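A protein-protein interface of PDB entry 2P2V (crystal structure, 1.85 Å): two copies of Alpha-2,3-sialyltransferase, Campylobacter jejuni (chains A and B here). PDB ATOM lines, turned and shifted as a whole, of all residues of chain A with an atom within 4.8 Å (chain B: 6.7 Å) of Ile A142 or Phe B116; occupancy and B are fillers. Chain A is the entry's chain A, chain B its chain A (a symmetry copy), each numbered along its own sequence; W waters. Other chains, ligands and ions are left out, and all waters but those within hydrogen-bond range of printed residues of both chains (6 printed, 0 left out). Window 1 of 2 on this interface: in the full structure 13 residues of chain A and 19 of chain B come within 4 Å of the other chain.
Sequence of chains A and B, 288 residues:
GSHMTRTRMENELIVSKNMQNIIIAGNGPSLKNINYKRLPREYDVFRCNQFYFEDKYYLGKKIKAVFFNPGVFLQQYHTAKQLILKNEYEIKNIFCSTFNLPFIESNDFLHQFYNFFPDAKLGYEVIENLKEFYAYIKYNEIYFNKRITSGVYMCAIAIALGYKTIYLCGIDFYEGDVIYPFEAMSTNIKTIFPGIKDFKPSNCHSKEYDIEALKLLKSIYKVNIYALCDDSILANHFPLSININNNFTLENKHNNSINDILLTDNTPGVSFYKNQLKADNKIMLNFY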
ATOM      1  N   LEU A 101       0.763   9.743 -19.819  1.00  0.00           N
ATOM      2  CA  LEU A 101       0.088   9.597 -18.562  1.00  0.00           C
ATOM      3  C   LEU A 101       0.428   8.181 -18.091  1.00  0.00           C
ATOM      4  O   LEU A 101       0.351   7.250 -18.876  1.00  0.00           O
ATOM      5  CB  LEU A 101      -1.428   9.691 -18.762  1.00  0.00           C
ATOM      6  CG  LEU A 101      -1.914  11.119 -19.085  1.00  0.00           C
ATOM      7  CD1 LEU A 101      -3.339  11.154 -19.465  1.00  0.00           C
ATOM      8  CD2 LEU A 101      -1.698  11.890 -17.825  1.00  0.00           C
ATOM      9  N   PRO A 102       0.891   8.059 -16.859  1.00  0.00           N
ATOM     10  CA  PRO A 102       1.515   6.790 -16.412  1.00  0.00           C
ATOM     11  C   PRO A 102       0.549   5.628 -16.168  1.00  0.00           C
ATOM     12  O   PRO A 102       1.009   4.484 -15.953  1.00  0.00           O
ATOM     13  CB  PRO A 102       2.181   7.163 -15.115  1.00  0.00           C
ATOM     14  CG  PRO A 102       1.320   8.346 -14.567  1.00  0.00           C
ATOM     15  CD  PRO A 102       1.002   9.121 -15.836  1.00  0.00           C
ATOM     16  N   PHE A 103      -0.743   5.920 -16.175  1.00  0.00           N
ATOM     17  CA  PHE A 103      -1.772   4.883 -16.155  1.00  0.00           C
ATOM     18  C   PHE A 103      -2.199   4.459 -17.553  1.00  0.00           C
ATOM     19  O   PHE A 103      -3.094   3.596 -17.717  1.00  0.00           O
ATOM     20  CB  PHE A 103      -2.960   5.298 -15.251  1.00  0.00           C
ATOM     21  CG  PHE A 103      -3.653   6.566 -15.707  1.00  0.00           C
ATOM     22  CD1 PHE A 103      -3.185   7.806 -15.265  1.00  0.00           C
ATOM     23  CD2 PHE A 103      -4.716   6.515 -16.611  1.00  0.00           C
ATOM     24  CE1 PHE A 103      -3.811   9.017 -15.694  1.00  0.00           C
ATOM     25  CE2 PHE A 103      -5.341   7.727 -17.095  1.00  0.00           C
ATOM     26  CZ  PHE A 103      -4.872   8.987 -16.629  1.00  0.00           C
ATOM     27  N   LYS A 138      -6.230  16.083 -21.025  1.00  0.00           N
ATOM     28  CA  LYS A 138      -5.755  15.445 -19.774  1.00  0.00           C
ATOM     29  C   LYS A 138      -6.730  15.584 -18.635  1.00  0.00           C
ATOM     30  O   LYS A 138      -6.929  14.606 -17.878  1.00  0.00           O
ATOM     31  CB  LYS A 138      -4.352  15.948 -19.382  1.00  0.00           C
ATOM     32  CG  LYS A 138      -3.301  15.598 -20.469  1.00  0.00           C
ATOM     33  CD  LYS A 138      -1.942  15.572 -19.833  1.00  0.00           C
ATOM     34  CE  LYS A 138      -1.097  14.589 -20.578  1.00  0.00           C
ATOM     35  NZ  LYS A 138       0.204  14.366 -19.976  1.00  0.00           N
ATOM     36  N   TYR A 139      -7.360  16.754 -18.514  1.00  0.00           N
ATOM     37  CA  TYR A 139      -8.331  16.997 -17.455  1.00  0.00           C
ATOM     38  C   TYR A 139      -9.495  16.003 -17.643  1.00  0.00           C
ATOM     39  O   TYR A 139      -9.926  15.337 -16.698  1.00  0.00           O
ATOM     40  CB  TYR A 139      -8.875  18.438 -17.527  1.00  0.00           C
ATOM     41  CG  TYR A 139      -9.902  18.763 -16.463  1.00  0.00           C
ATOM     42  CD1 TYR A 139      -9.617  18.570 -15.105  1.00  0.00           C
ATOM     43  CD2 TYR A 139     -11.167  19.318 -16.800  1.00  0.00           C
ATOM     44  CE1 TYR A 139     -10.556  18.887 -14.114  1.00  0.00           C
ATOM     45  CE2 TYR A 139     -12.113  19.642 -15.793  1.00  0.00           C
ATOM     46  CZ  TYR A 139     -11.813  19.402 -14.465  1.00  0.00           C
ATOM     47  OH  TYR A 139     -12.702  19.679 -13.433  1.00  0.00           O
ATOM     48  N   ASN A 140      -9.992  15.902 -18.857  1.00  0.00           N
ATOM     49  CA  ASN A 140     -11.124  14.946 -19.093  1.00  0.00           C
ATOM     50  C   ASN A 140     -10.768  13.477 -18.955  1.00  0.00           C
ATOM     51  O   ASN A 140     -11.560  12.702 -18.375  1.00  0.00           O
ATOM     52  CB  ASN A 140     -11.733  15.159 -20.446  1.00  0.00           C
ATOM     53  CG  ASN A 140     -12.574  16.362 -20.491  1.00  0.00           C
ATOM     54  OD1 ASN A 140     -13.514  16.502 -19.726  1.00  0.00           O
ATOM     55  ND2 ASN A 140     -12.229  17.267 -21.354  1.00  0.00           N
ATOM     56  N   GLU A 141      -9.574  13.091 -19.402  1.00  0.00           N
ATOM     57  CA  GLU A 141      -9.075  11.734 -19.137  1.00  0.00           C
ATOM     58  C   GLU A 141      -8.965  11.443 -17.669  1.00  0.00           C
ATOM     59  O   GLU A 141      -9.565  10.427 -17.116  1.00  0.00           O
ATOM     60  CB  GLU A 141      -7.711  11.561 -19.826  1.00  0.00           C
ATOM     61  CG  GLU A 141      -7.005  10.233 -19.510  1.00  0.00           C
ATOM     62  CD  GLU A 141      -7.556   9.068 -20.301  1.00  0.00           C
ATOM     63  OE1 GLU A 141      -7.677   9.150 -21.531  1.00  0.00           O
ATOM     64  OE2 GLU A 141      -7.864   8.031 -19.668  1.00  0.00           O
ATOM     65  N   ILE A 142      -8.188  12.246 -16.936  1.00  0.00           N
ATOM     66  CA  ILE A 142      -7.938  11.918 -15.513  1.00  0.00           C
ATOM     67  C   ILE A 142      -9.174  11.955 -14.632  1.00  0.00           C
ATOM     68  O   ILE A 142      -9.404  11.034 -13.789  1.00  0.00           O
ATOM     69  CB  ILE A 142      -6.843  12.918 -14.886  1.00  0.00           C
ATOM     70  CG1 ILE A 142      -5.485  12.656 -15.592  1.00  0.00           C
ATOM     71  CG2 ILE A 142      -6.730  12.725 -13.362  1.00  0.00           C
ATOM     72  CD1 ILE A 142      -4.500  13.906 -15.612  1.00  0.00           C
ATOM     73  N   TYR A 143      -9.953  13.018 -14.757  1.00  0.00           N
ATOM     74  CA  TYR A 143     -11.031  13.233 -13.800  1.00  0.00           C
ATOM     75  C   TYR A 143     -12.361  12.636 -14.276  1.00  0.00           C
ATOM     76  O   TYR A 143     -13.301  12.470 -13.472  1.00  0.00           O
ATOM     77  CB  TYR A 143     -11.220  14.705 -13.553  1.00  0.00           C
ATOM     78  CG  TYR A 143     -10.061  15.290 -12.746  1.00  0.00           C
ATOM     79  CD1 TYR A 143     -10.075  15.288 -11.355  1.00  0.00           C
ATOM     80  CD2 TYR A 143      -8.922  15.800 -13.396  1.00  0.00           C
ATOM     81  CE1 TYR A 143      -9.004  15.793 -10.614  1.00  0.00           C
ATOM     82  CE2 TYR A 143      -7.874  16.353 -12.671  1.00  0.00           C
ATOM     83  CZ  TYR A 143      -7.902  16.364 -11.322  1.00  0.00           C
ATOM     84  OH  TYR A 143      -6.849  16.929 -10.675  1.00  0.00           O
ATOM     85  N   PHE A 144     -12.467  12.348 -15.551  1.00  0.00           N
ATOM     86  CA  PHE A 144     -13.798  11.948 -16.071  1.00  0.00           C
ATOM     87  C   PHE A 144     -13.747  10.687 -16.905  1.00  0.00           C
ATOM     88  O   PHE A 144     -14.810  10.255 -17.385  1.00  0.00           O
ATOM     89  CB  PHE A 144     -14.493  13.078 -16.863  1.00  0.00           C
ATOM     90  CG  PHE A 144     -14.747  14.338 -16.050  1.00  0.00           C
ATOM     91  CD1 PHE A 144     -15.829  14.435 -15.158  1.00  0.00           C
ATOM     92  CD2 PHE A 144     -13.908  15.429 -16.168  1.00  0.00           C
ATOM     93  CE1 PHE A 144     -16.060  15.593 -14.406  1.00  0.00           C
ATOM     94  CE2 PHE A 144     -14.115  16.572 -15.412  1.00  0.00           C
ATOM     95  CZ  PHE A 144     -15.187  16.667 -14.524  1.00  0.00           C
ATOM     96  N   ASN A 145     -12.550  10.126 -17.129  1.00  0.00           N
ATOM     97  CA  ASN A 145     -12.407   8.875 -17.884  1.00  0.00           C
ATOM     98  C   ASN A 145     -12.949   8.984 -19.290  1.00  0.00           C
ATOM     99  O   ASN A 145     -13.578   8.071 -19.806  1.00  0.00           O
ATOM    100  CB  ASN A 145     -13.091   7.737 -17.096  1.00  0.00           C
ATOM    101  CG  ASN A 145     -12.773   6.366 -17.649  1.00  0.00           C
ATOM    102  OD1 ASN A 145     -11.645   6.081 -18.092  1.00  0.00           O
ATOM    103  ND2 ASN A 145     -13.782   5.486 -17.626  1.00  0.00           N
ATOM    104  N   LEU B  74      -4.527  17.376  -6.267  1.00  0.00           N
ATOM    105  CA  LEU B  74      -5.456  16.749  -7.207  1.00  0.00           C
ATOM    106  C   LEU B  74      -6.863  17.314  -7.095  1.00  0.00           C
ATOM    107  O   LEU B  74      -7.480  17.628  -8.109  1.00  0.00           O
ATOM    108  CB  LEU B  74      -5.484  15.205  -6.951  1.00  0.00           C
ATOM    109  CG  LEU B  74      -6.381  14.381  -7.907  1.00  0.00           C
ATOM    110  CD1 LEU B  74      -5.693  14.045  -9.182  1.00  0.00           C
ATOM    111  CD2 LEU B  74      -6.672  13.048  -7.157  1.00  0.00           C
ATOM    112  N   TYR B  77      -6.913  21.262  -7.945  1.00  0.00           N
ATOM    113  CA  TYR B  77      -6.804  21.511  -9.414  1.00  0.00           C
ATOM    114  C   TYR B  77      -8.173  21.372 -10.086  1.00  0.00           C
ATOM    115  O   TYR B  77      -8.601  22.200 -10.839  1.00  0.00           O
ATOM    116  CB  TYR B  77      -5.804  20.523 -10.020  1.00  0.00           C
ATOM    117  CG  TYR B  77      -5.546  20.721 -11.499  1.00  0.00           C
ATOM    118  CD1 TYR B  77      -4.646  21.706 -11.940  1.00  0.00           C
ATOM    119  CD2 TYR B  77      -6.210  19.967 -12.454  1.00  0.00           C
ATOM    120  CE1 TYR B  77      -4.418  21.895 -13.313  1.00  0.00           C
ATOM    121  CE2 TYR B  77      -5.973  20.145 -13.849  1.00  0.00           C
ATOM    122  CZ  TYR B  77      -5.056  21.082 -14.238  1.00  0.00           C
ATOM    123  OH  TYR B  77      -4.865  21.194 -15.592  1.00  0.00           O
ATOM    124  N   ASP B 108       7.934  10.695  -6.875  1.00  0.00           N
ATOM    125  CA  ASP B 108       6.929  10.449  -7.899  1.00  0.00           C
ATOM    126  C   ASP B 108       5.995  11.627  -8.094  1.00  0.00           C
ATOM    127  O   ASP B 108       5.617  11.885  -9.195  1.00  0.00           O
ATOM    128  CB  ASP B 108       6.065   9.226  -7.596  1.00  0.00           C
ATOM    129  CG  ASP B 108       6.760   7.873  -7.977  1.00  0.00           C
ATOM    130  OD1 ASP B 108       7.730   7.849  -8.776  1.00  0.00           O
ATOM    131  OD2 ASP B 108       6.287   6.820  -7.469  1.00  0.00           O
ATOM    132  N   PHE B 109       5.591  12.289  -7.015  1.00  0.00           N
ATOM    133  CA  PHE B 109       4.724  13.473  -7.127  1.00  0.00           C
ATOM    134  C   PHE B 109       5.415  14.485  -8.033  1.00  0.00           C
ATOM    135  O   PHE B 109       4.794  15.000  -8.977  1.00  0.00           O
ATOM    136  CB  PHE B 109       4.488  14.132  -5.774  1.00  0.00           C
ATOM    137  CG  PHE B 109       3.639  15.385  -5.861  1.00  0.00           C
ATOM    138  CD1 PHE B 109       2.248  15.311  -5.900  1.00  0.00           C
ATOM    139  CD2 PHE B 109       4.233  16.645  -5.930  1.00  0.00           C
ATOM    140  CE1 PHE B 109       1.450  16.487  -6.045  1.00  0.00           C
ATOM    141  CE2 PHE B 109       3.463  17.826  -6.077  1.00  0.00           C
ATOM    142  CZ  PHE B 109       2.081  17.770  -6.120  1.00  0.00           C
ATOM    143  N   GLN B 112       5.941  13.285 -11.858  1.00  0.00           N
ATOM    144  CA  GLN B 112       4.719  13.115 -12.646  1.00  0.00           C
ATOM    145  C   GLN B 112       3.867  14.349 -12.618  1.00  0.00           C
ATOM    146  O   GLN B 112       2.868  14.372 -13.265  1.00  0.00           O
ATOM    147  CB  GLN B 112       3.858  11.979 -12.064  1.00  0.00           C
ATOM    148  CG  GLN B 112       4.638  10.716 -12.126  1.00  0.00           C
ATOM    149  CD  GLN B 112       3.843   9.529 -11.625  1.00  0.00           C
ATOM    150  OE1 GLN B 112       4.059   8.406 -12.081  1.00  0.00           O
ATOM    151  NE2 GLN B 112       2.931   9.768 -10.670  1.00  0.00           N
ATOM    152  N   PHE B 113       4.274  15.382 -11.874  1.00  0.00           N
ATOM    153  CA  PHE B 113       3.442  16.573 -11.765  1.00  0.00           C
ATOM    154  C   PHE B 113       2.922  17.099 -13.071  1.00  0.00           C
ATOM    155  O   PHE B 113       1.711  17.277 -13.233  1.00  0.00           O
ATOM    156  CB  PHE B 113       4.190  17.711 -10.996  1.00  0.00           C
ATOM    157  CG  PHE B 113       3.329  18.887 -10.756  1.00  0.00           C
ATOM    158  CD1 PHE B 113       2.437  18.925  -9.679  1.00  0.00           C
ATOM    159  CD2 PHE B 113       3.354  19.972 -11.646  1.00  0.00           C
ATOM    160  CE1 PHE B 113       1.612  20.008  -9.447  1.00  0.00           C
ATOM    161  CE2 PHE B 113       2.525  21.009 -11.438  1.00  0.00           C
ATOM    162  CZ  PHE B 113       1.672  21.086 -10.320  1.00  0.00           C
ATOM    163  N   TYR B 114       3.819  17.469 -14.006  1.00  0.00           N
ATOM    164  CA  TYR B 114       3.355  18.023 -15.236  1.00  0.00           C
ATOM    165  C   TYR B 114       2.644  17.029 -16.118  1.00  0.00           C
ATOM    166  O   TYR B 114       1.882  17.414 -16.995  1.00  0.00           O
ATOM    167  CB  TYR B 114       4.550  18.636 -15.983  1.00  0.00           C
ATOM    168  CG  TYR B 114       5.044  19.865 -15.284  1.00  0.00           C
ATOM    169  CD1 TYR B 114       4.184  20.929 -15.044  1.00  0.00           C
ATOM    170  CD2 TYR B 114       6.381  19.956 -14.858  1.00  0.00           C
ATOM    171  CE1 TYR B 114       4.663  22.102 -14.381  1.00  0.00           C
ATOM    172  CE2 TYR B 114       6.856  21.105 -14.183  1.00  0.00           C
ATOM    173  CZ  TYR B 114       5.995  22.163 -13.959  1.00  0.00           C
ATOM    174  OH  TYR B 114       6.431  23.326 -13.321  1.00  0.00           O
ATOM    175  N   ASN B 115       2.868  15.730 -15.874  1.00  0.00           N
ATOM    176  CA  ASN B 115       2.150  14.710 -16.634  1.00  0.00           C
ATOM    177  C   ASN B 115       0.649  14.810 -16.342  1.00  0.00           C
ATOM    178  O   ASN B 115      -0.150  14.674 -17.242  1.00  0.00           O
ATOM    179  CB  ASN B 115       2.681  13.280 -16.275  1.00  0.00           C
ATOM    180  CG  ASN B 115       4.173  13.121 -16.546  1.00  0.00           C
ATOM    181  OD1 ASN B 115       5.005  13.533 -15.765  1.00  0.00           O
ATOM    182  ND2 ASN B 115       4.498  12.537 -17.634  1.00  0.00           N
ATOM    183  N   PHE B 116       0.298  14.938 -15.060  1.00  0.00           N
ATOM    184  CA  PHE B 116      -1.069  15.111 -14.617  1.00  0.00           C
ATOM    185  C   PHE B 116      -1.626  16.520 -14.782  1.00  0.00           C
ATOM    186  O   PHE B 116      -2.806  16.652 -15.050  1.00  0.00           O
ATOM    187  CB  PHE B 116      -1.230  14.682 -13.189  1.00  0.00           C
ATOM    188  CG  PHE B 116      -1.191  13.175 -13.025  1.00  0.00           C
ATOM    189  CD1 PHE B 116      -2.385  12.449 -13.137  1.00  0.00           C
ATOM    190  CD2 PHE B 116      -0.016  12.522 -12.799  1.00  0.00           C
ATOM    191  CE1 PHE B 116      -2.415  11.004 -12.956  1.00  0.00           C
ATOM    192  CE2 PHE B 116      -0.019  11.058 -12.632  1.00  0.00           C
ATOM    193  CZ  PHE B 116      -1.248  10.347 -12.738  1.00  0.00           C
ATOM    194  N   PHE B 117      -0.786  17.549 -14.604  1.00  0.00           N
ATOM    195  CA  PHE B 117      -1.287  18.908 -14.497  1.00  0.00           C
ATOM    196  C   PHE B 117      -0.462  19.777 -15.457  1.00  0.00           C
ATOM    197  O   PHE B 117       0.299  20.569 -14.943  1.00  0.00           O
ATOM    198  CB  PHE B 117      -1.112  19.382 -13.066  1.00  0.00           C
ATOM    199  CG  PHE B 117      -1.683  18.366 -11.996  1.00  0.00           C
ATOM    200  CD1 PHE B 117      -3.068  18.106 -11.958  1.00  0.00           C
ATOM    201  CD2 PHE B 117      -0.855  17.774 -11.131  1.00  0.00           C
ATOM    202  CE1 PHE B 117      -3.572  17.160 -11.015  1.00  0.00           C
ATOM    203  CE2 PHE B 117      -1.320  16.835 -10.162  1.00  0.00           C
ATOM    204  CZ  PHE B 117      -2.693  16.580 -10.143  1.00  0.00           C
ATOM    205  N   PRO B 118      -0.602  19.590 -16.797  1.00  0.00           N
ATOM    206  CA  PRO B 118       0.324  20.168 -17.774  1.00  0.00           C
ATOM    207  C   PRO B 118       0.368  21.681 -17.800  1.00  0.00           C
ATOM    208  O   PRO B 118       1.381  22.249 -18.199  1.00  0.00           O
ATOM    209  CB  PRO B 118      -0.149  19.568 -19.103  1.00  0.00           C
ATOM    210  CG  PRO B 118      -1.563  19.162 -18.873  1.00  0.00           C
ATOM    211  CD  PRO B 118      -1.627  18.755 -17.461  1.00  0.00           C
ATOM    212  N   ASP B 119      -0.716  22.309 -17.380  1.00  0.00           N
ATOM    213  CA  ASP B 119      -0.827  23.778 -17.336  1.00  0.00           C
ATOM    214  C   ASP B 119      -0.663  24.372 -15.957  1.00  0.00           C
ATOM    215  O   ASP B 119      -0.829  25.598 -15.787  1.00  0.00           O
ATOM    216  CB  ASP B 119      -2.134  24.227 -17.981  1.00  0.00           C
ATOM    217  CG  ASP B 119      -3.373  23.734 -17.282  1.00  0.00           C
ATOM    218  OD1 ASP B 119      -3.278  22.882 -16.352  1.00  0.00           O
ATOM    219  OD2 ASP B 119      -4.445  24.196 -17.688  1.00  0.00           O
ATOM    220  N   ASP B 265     -14.040  11.575  -8.675  1.00  0.00           N
ATOM    221  CA  ASP B 265     -14.502  10.206  -8.954  1.00  0.00           C
ATOM    222  C   ASP B 265     -13.332   9.233  -9.076  1.00  0.00           C
ATOM    223  O   ASP B 265     -12.248   9.595  -9.542  1.00  0.00           O
ATOM    224  CB  ASP B 265     -15.295  10.204 -10.242  1.00  0.00           C
ATOM    225  CG  ASP B 265     -16.690  10.799 -10.073  1.00  0.00           C
ATOM    226  OD1 ASP B 265     -17.173  10.866  -8.923  1.00  0.00           O
ATOM    227  OD2 ASP B 265     -17.307  11.185 -11.086  1.00  0.00           O
ATOM    228  N   ASN B 266     -13.565   7.987  -8.680  1.00  0.00           N
ATOM    229  CA  ASN B 266     -12.594   6.929  -8.770  1.00  0.00           C
ATOM    230  C   ASN B 266     -12.367   6.410 -10.208  1.00  0.00           C
ATOM    231  O   ASN B 266     -12.598   5.227 -10.524  1.00  0.00           O
ATOM    232  CB  ASN B 266     -13.049   5.805  -7.851  1.00  0.00           C
ATOM    233  CG  ASN B 266     -11.990   4.749  -7.650  1.00  0.00           C
ATOM    234  OD1 ASN B 266     -12.243   3.549  -7.880  1.00  0.00           O
ATOM    235  ND2 ASN B 266     -10.808   5.167  -7.181  1.00  0.00           N
ATOM    236  N   THR B 267     -11.926   7.291 -11.113  1.00  0.00           N
ATOM    237  CA  THR B 267     -11.521   6.871 -12.450  1.00  0.00           C
ATOM    238  C   THR B 267     -10.183   6.088 -12.447  1.00  0.00           C
ATOM    239  O   THR B 267      -9.502   5.989 -11.406  1.00  0.00           O
ATOM    240  CB  THR B 267     -11.335   8.110 -13.341  1.00  0.00           C
ATOM    241  OG1 THR B 267     -10.269   8.881 -12.781  1.00  0.00           O
ATOM    242  CG2 THR B 267     -12.606   8.930 -13.403  1.00  0.00           C
ATOM    243  N   PRO B 268      -9.799   5.484 -13.582  1.00  0.00           N
ATOM    244  CA  PRO B 268      -8.506   4.795 -13.596  1.00  0.00           C
ATOM    245  C   PRO B 268      -7.362   5.772 -13.259  1.00  0.00           C
ATOM    246  O   PRO B 268      -6.475   5.442 -12.522  1.00  0.00           O
ATOM    247  CB  PRO B 268      -8.401   4.288 -15.016  1.00  0.00           C
ATOM    248  CG  PRO B 268      -9.823   4.016 -15.377  1.00  0.00           C
ATOM    249  CD  PRO B 268     -10.526   5.264 -14.846  1.00  0.00           C
ATOM    250  N   GLY B 269      -7.455   6.995 -13.745  1.00  0.00           N
ATOM    251  CA  GLY B 269      -6.363   7.965 -13.497  1.00  0.00           C
ATOM    252  C   GLY B 269      -6.300   8.462 -12.065  1.00  0.00           C
ATOM    253  O   GLY B 269      -5.228   8.529 -11.497  1.00  0.00           O
ATOM    254  N   VAL B 270      -7.452   8.816 -11.494  1.00  0.00           N
ATOM    255  CA  VAL B 270      -7.537   9.243 -10.097  1.00  0.00           C
ATOM    256  C   VAL B 270      -7.116   8.081  -9.226  1.00  0.00           C
ATOM    257  O   VAL B 270      -6.374   8.277  -8.263  1.00  0.00           O
ATOM    258  CB  VAL B 270      -8.966   9.755  -9.700  1.00  0.00           C
ATOM    259  CG1 VAL B 270      -9.095   9.906  -8.209  1.00  0.00           C
ATOM    260  CG2 VAL B 270      -9.234  11.146 -10.305  1.00  0.00           C
ATOM    261  N   SER B 271      -7.597   6.854  -9.510  1.00  0.00           N
ATOM    262  CA  SER B 271      -7.185   5.743  -8.614  1.00  0.00           C
ATOM    263  C   SER B 271      -5.686   5.486  -8.647  1.00  0.00           C
ATOM    264  O   SER B 271      -5.096   5.235  -7.624  1.00  0.00           O
ATOM    265  CB  SER B 271      -8.027   4.430  -8.795  1.00  0.00           C
ATOM    266  OG  SER B 271      -8.226   4.202 -10.153  1.00  0.00           O
ATOM    267  N   PHE B 272      -5.088   5.523  -9.840  1.00  0.00           N
ATOM    268  CA  PHE B 272      -3.679   5.374 -10.028  1.00  0.00           C
ATOM    269  C   PHE B 272      -2.956   6.419  -9.169  1.00  0.00           C
ATOM    270  O   PHE B 272      -2.017   6.114  -8.418  1.00  0.00           O
ATOM    271  CB  PHE B 272      -3.308   5.583 -11.528  1.00  0.00           C
ATOM    272  CG  PHE B 272      -1.821   5.462 -11.770  1.00  0.00           C
ATOM    273  CD1 PHE B 272      -0.989   6.558 -11.503  1.00  0.00           C
ATOM    274  CD2 PHE B 272      -1.259   4.249 -12.189  1.00  0.00           C
ATOM    275  CE1 PHE B 272       0.379   6.459 -11.638  1.00  0.00           C
ATOM    276  CE2 PHE B 272       0.115   4.156 -12.391  1.00  0.00           C
ATOM    277  CZ  PHE B 272       0.942   5.265 -12.082  1.00  0.00           C
ATOM    278  N   TYR B 273      -3.392   7.667  -9.335  1.00  0.00           N
ATOM    279  CA  TYR B 273      -2.784   8.814  -8.616  1.00  0.00           C
ATOM    280  C   TYR B 273      -2.841   8.691  -7.097  1.00  0.00           C
ATOM    281  O   TYR B 273      -1.805   8.817  -6.410  1.00  0.00           O
ATOM    282  CB  TYR B 273      -3.487  10.073  -9.083  1.00  0.00           C
ATOM    283  CG  TYR B 273      -2.852  11.332  -8.523  1.00  0.00           C
ATOM    284  CD1 TYR B 273      -2.020  12.120  -9.328  1.00  0.00           C
ATOM    285  CD2 TYR B 273      -3.076  11.725  -7.200  1.00  0.00           C
ATOM    286  CE1 TYR B 273      -1.414  13.287  -8.792  1.00  0.00           C
ATOM    287  CE2 TYR B 273      -2.511  12.887  -6.677  1.00  0.00           C
ATOM    288  CZ  TYR B 273      -1.675  13.639  -7.473  1.00  0.00           C
ATOM    289  OH  TYR B 273      -1.087  14.807  -6.982  1.00  0.00           O
ATOM    290  N   GLN B 276      -0.628   5.808  -5.629  1.00  0.00           N
ATOM    291  CA  GLN B 276       0.761   6.207  -5.547  1.00  0.00           C
ATOM    292  C   GLN B 276       0.973   7.174  -4.413  1.00  0.00           C
ATOM    293  O   GLN B 276       1.904   6.992  -3.628  1.00  0.00           O
ATOM    294  CB  GLN B 276       1.201   6.826  -6.853  1.00  0.00           C
ATOM    295  CG  GLN B 276       1.353   5.817  -7.927  1.00  0.00           C
ATOM    296  CD  GLN B 276       2.506   6.154  -8.827  1.00  0.00           C
ATOM    297  OE1 GLN B 276       2.778   7.330  -9.074  1.00  0.00           O
ATOM    298  NE2 GLN B 276       3.188   5.130  -9.338  1.00  0.00           N
HETATM  299  O   HOH W   1       1.942  16.543 -19.595  1.00  0.00           O
HETATM  300  O   HOH W   2       3.690   9.254 -18.122  1.00  0.00           O
HETATM  301  O   HOH W   3      -9.105   8.151 -15.797  1.00  0.00           O
HETATM  302  O   HOH W   4      -5.103  19.130 -17.382  1.00  0.00           O
HETATM  303  O   HOH W   5     -15.872  11.383 -13.357  1.00  0.00           O
HETATM  304  O   HOH W   6      -5.607  17.241 -15.700  1.00  0.00           O
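The backbone carbonyl oxygen (O) of Asn B115 lies within hydrogen-bond range of the side-chain amino group (NZ) of Lys A138 (2.8 Å).
The side-chain hydroxyl of Tyr A143 lies within hydrogen-bond range of the backbone carbonyl oxygen of Leu B74 (2.7 Å).
The backbone carbonyl oxygen of Ile A142 sits at hydrogen-bond distance from the side-chain hydroxyl of Thr B267 (2.5 Å).
OH of Tyr B77 is in hydrogen-bond range of OD1 of Asp B119 (2.4 Å).
The backbone carbonyl oxygen (O) of Pro B268 lies within hydrogen-bond range of the side-chain hydroxyl (OG) of Ser B271, at 3.2 Å.
The backbone carbonyl oxygen (O) of Gln B112 lies close to the side-chain amide oxygen (OD1) of Asn B115 (3.4 Å).
CE2 of Phe B116 touches CG of Pro A102, 3.6 Å away.
CG of Pro A102 touches CE1 of Phe B272 (3.6 Å).
Phe A103 touches Phe B116.
Phe B272 touches Phe A103 (CD2 to CB, 3.7 Å).
CD1 of Ile A142 touches O of Phe B116, 3.3 Å away.
Val B270 touches Ile A142.
Tyr A143 touches Tyr B77.
Tyr A143 touches Phe B117 (OH to CE1, 3.3 Å).
Tyr A143 touches Thr B267.
CB of Asn A145 touches CG2 of Thr B267 (3.9 Å).
Of chain B, only Phe B116, Thr B267 and Val B270 come within 4 Å of Ile A142.
Of the printed residues of chain B, Pro A102 touches Gln B112, Phe B116 and Phe B272.
Of the printed residues of chain A, Phe B272 touches Pro A102 and Phe A103.
Of the printed residues of chain B, Phe A103 touches Phe B116, Gly B269 and Phe B272.
Of the printed residues of chain A, Phe B117 touches Tyr A143.
Asp B119 touches none of the printed residues of chain A.
The nearest residue of chain B that does not touch Ile A142 is Gly B269 (4.3 Å).
The nearest residue of chain A that does not touch Phe B116 is Leu A101 (4.6 Å).
The nearest printed residue of chain A that does not touch Phe B272 is Leu A101 (6.7 Å).
Of the 11 printed residues of chain A, 7 touch a printed residue of chain B.
Along chain A the printed residues that touch a printed residue of chain B span positions 101 to 145.
Of the 22 printed residues of chain B, 12 touch a printed residue of chain A.
Printed residues of chain B that touch a printed residue of chain A: Leu B74, Tyr B77, Gln B112, Asn B115, Phe B116, Phe B117, Pro B118, Thr B267, Pro B268, Gly B269, Val B270 and Phe B272.
Hydrophobic or aromatic side chains of chain B within 4 Å of the printed part of chain A: Leu B74, Tyr B77, Phe B116, Phe B117, Pro B118, Pro B268, Val B270 and Phe B272.
Among the printed residues, 18 pairs touch across the chains.
No position is printed for both chains.
Water W3 lies within hydrogen-bond range of O of Glu A141 (2.7 Å), N of Gly B269 (2.9 Å) and OG1 of Thr B267 (3.3 Å).
Water W4 lies within hydrogen-bond range of OH of Tyr B77 and N of Tyr A139.
Water W2 lies within hydrogen-bond range of the side-chain amide nitrogen of Asn B115 and the backbone NH of Leu A101.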
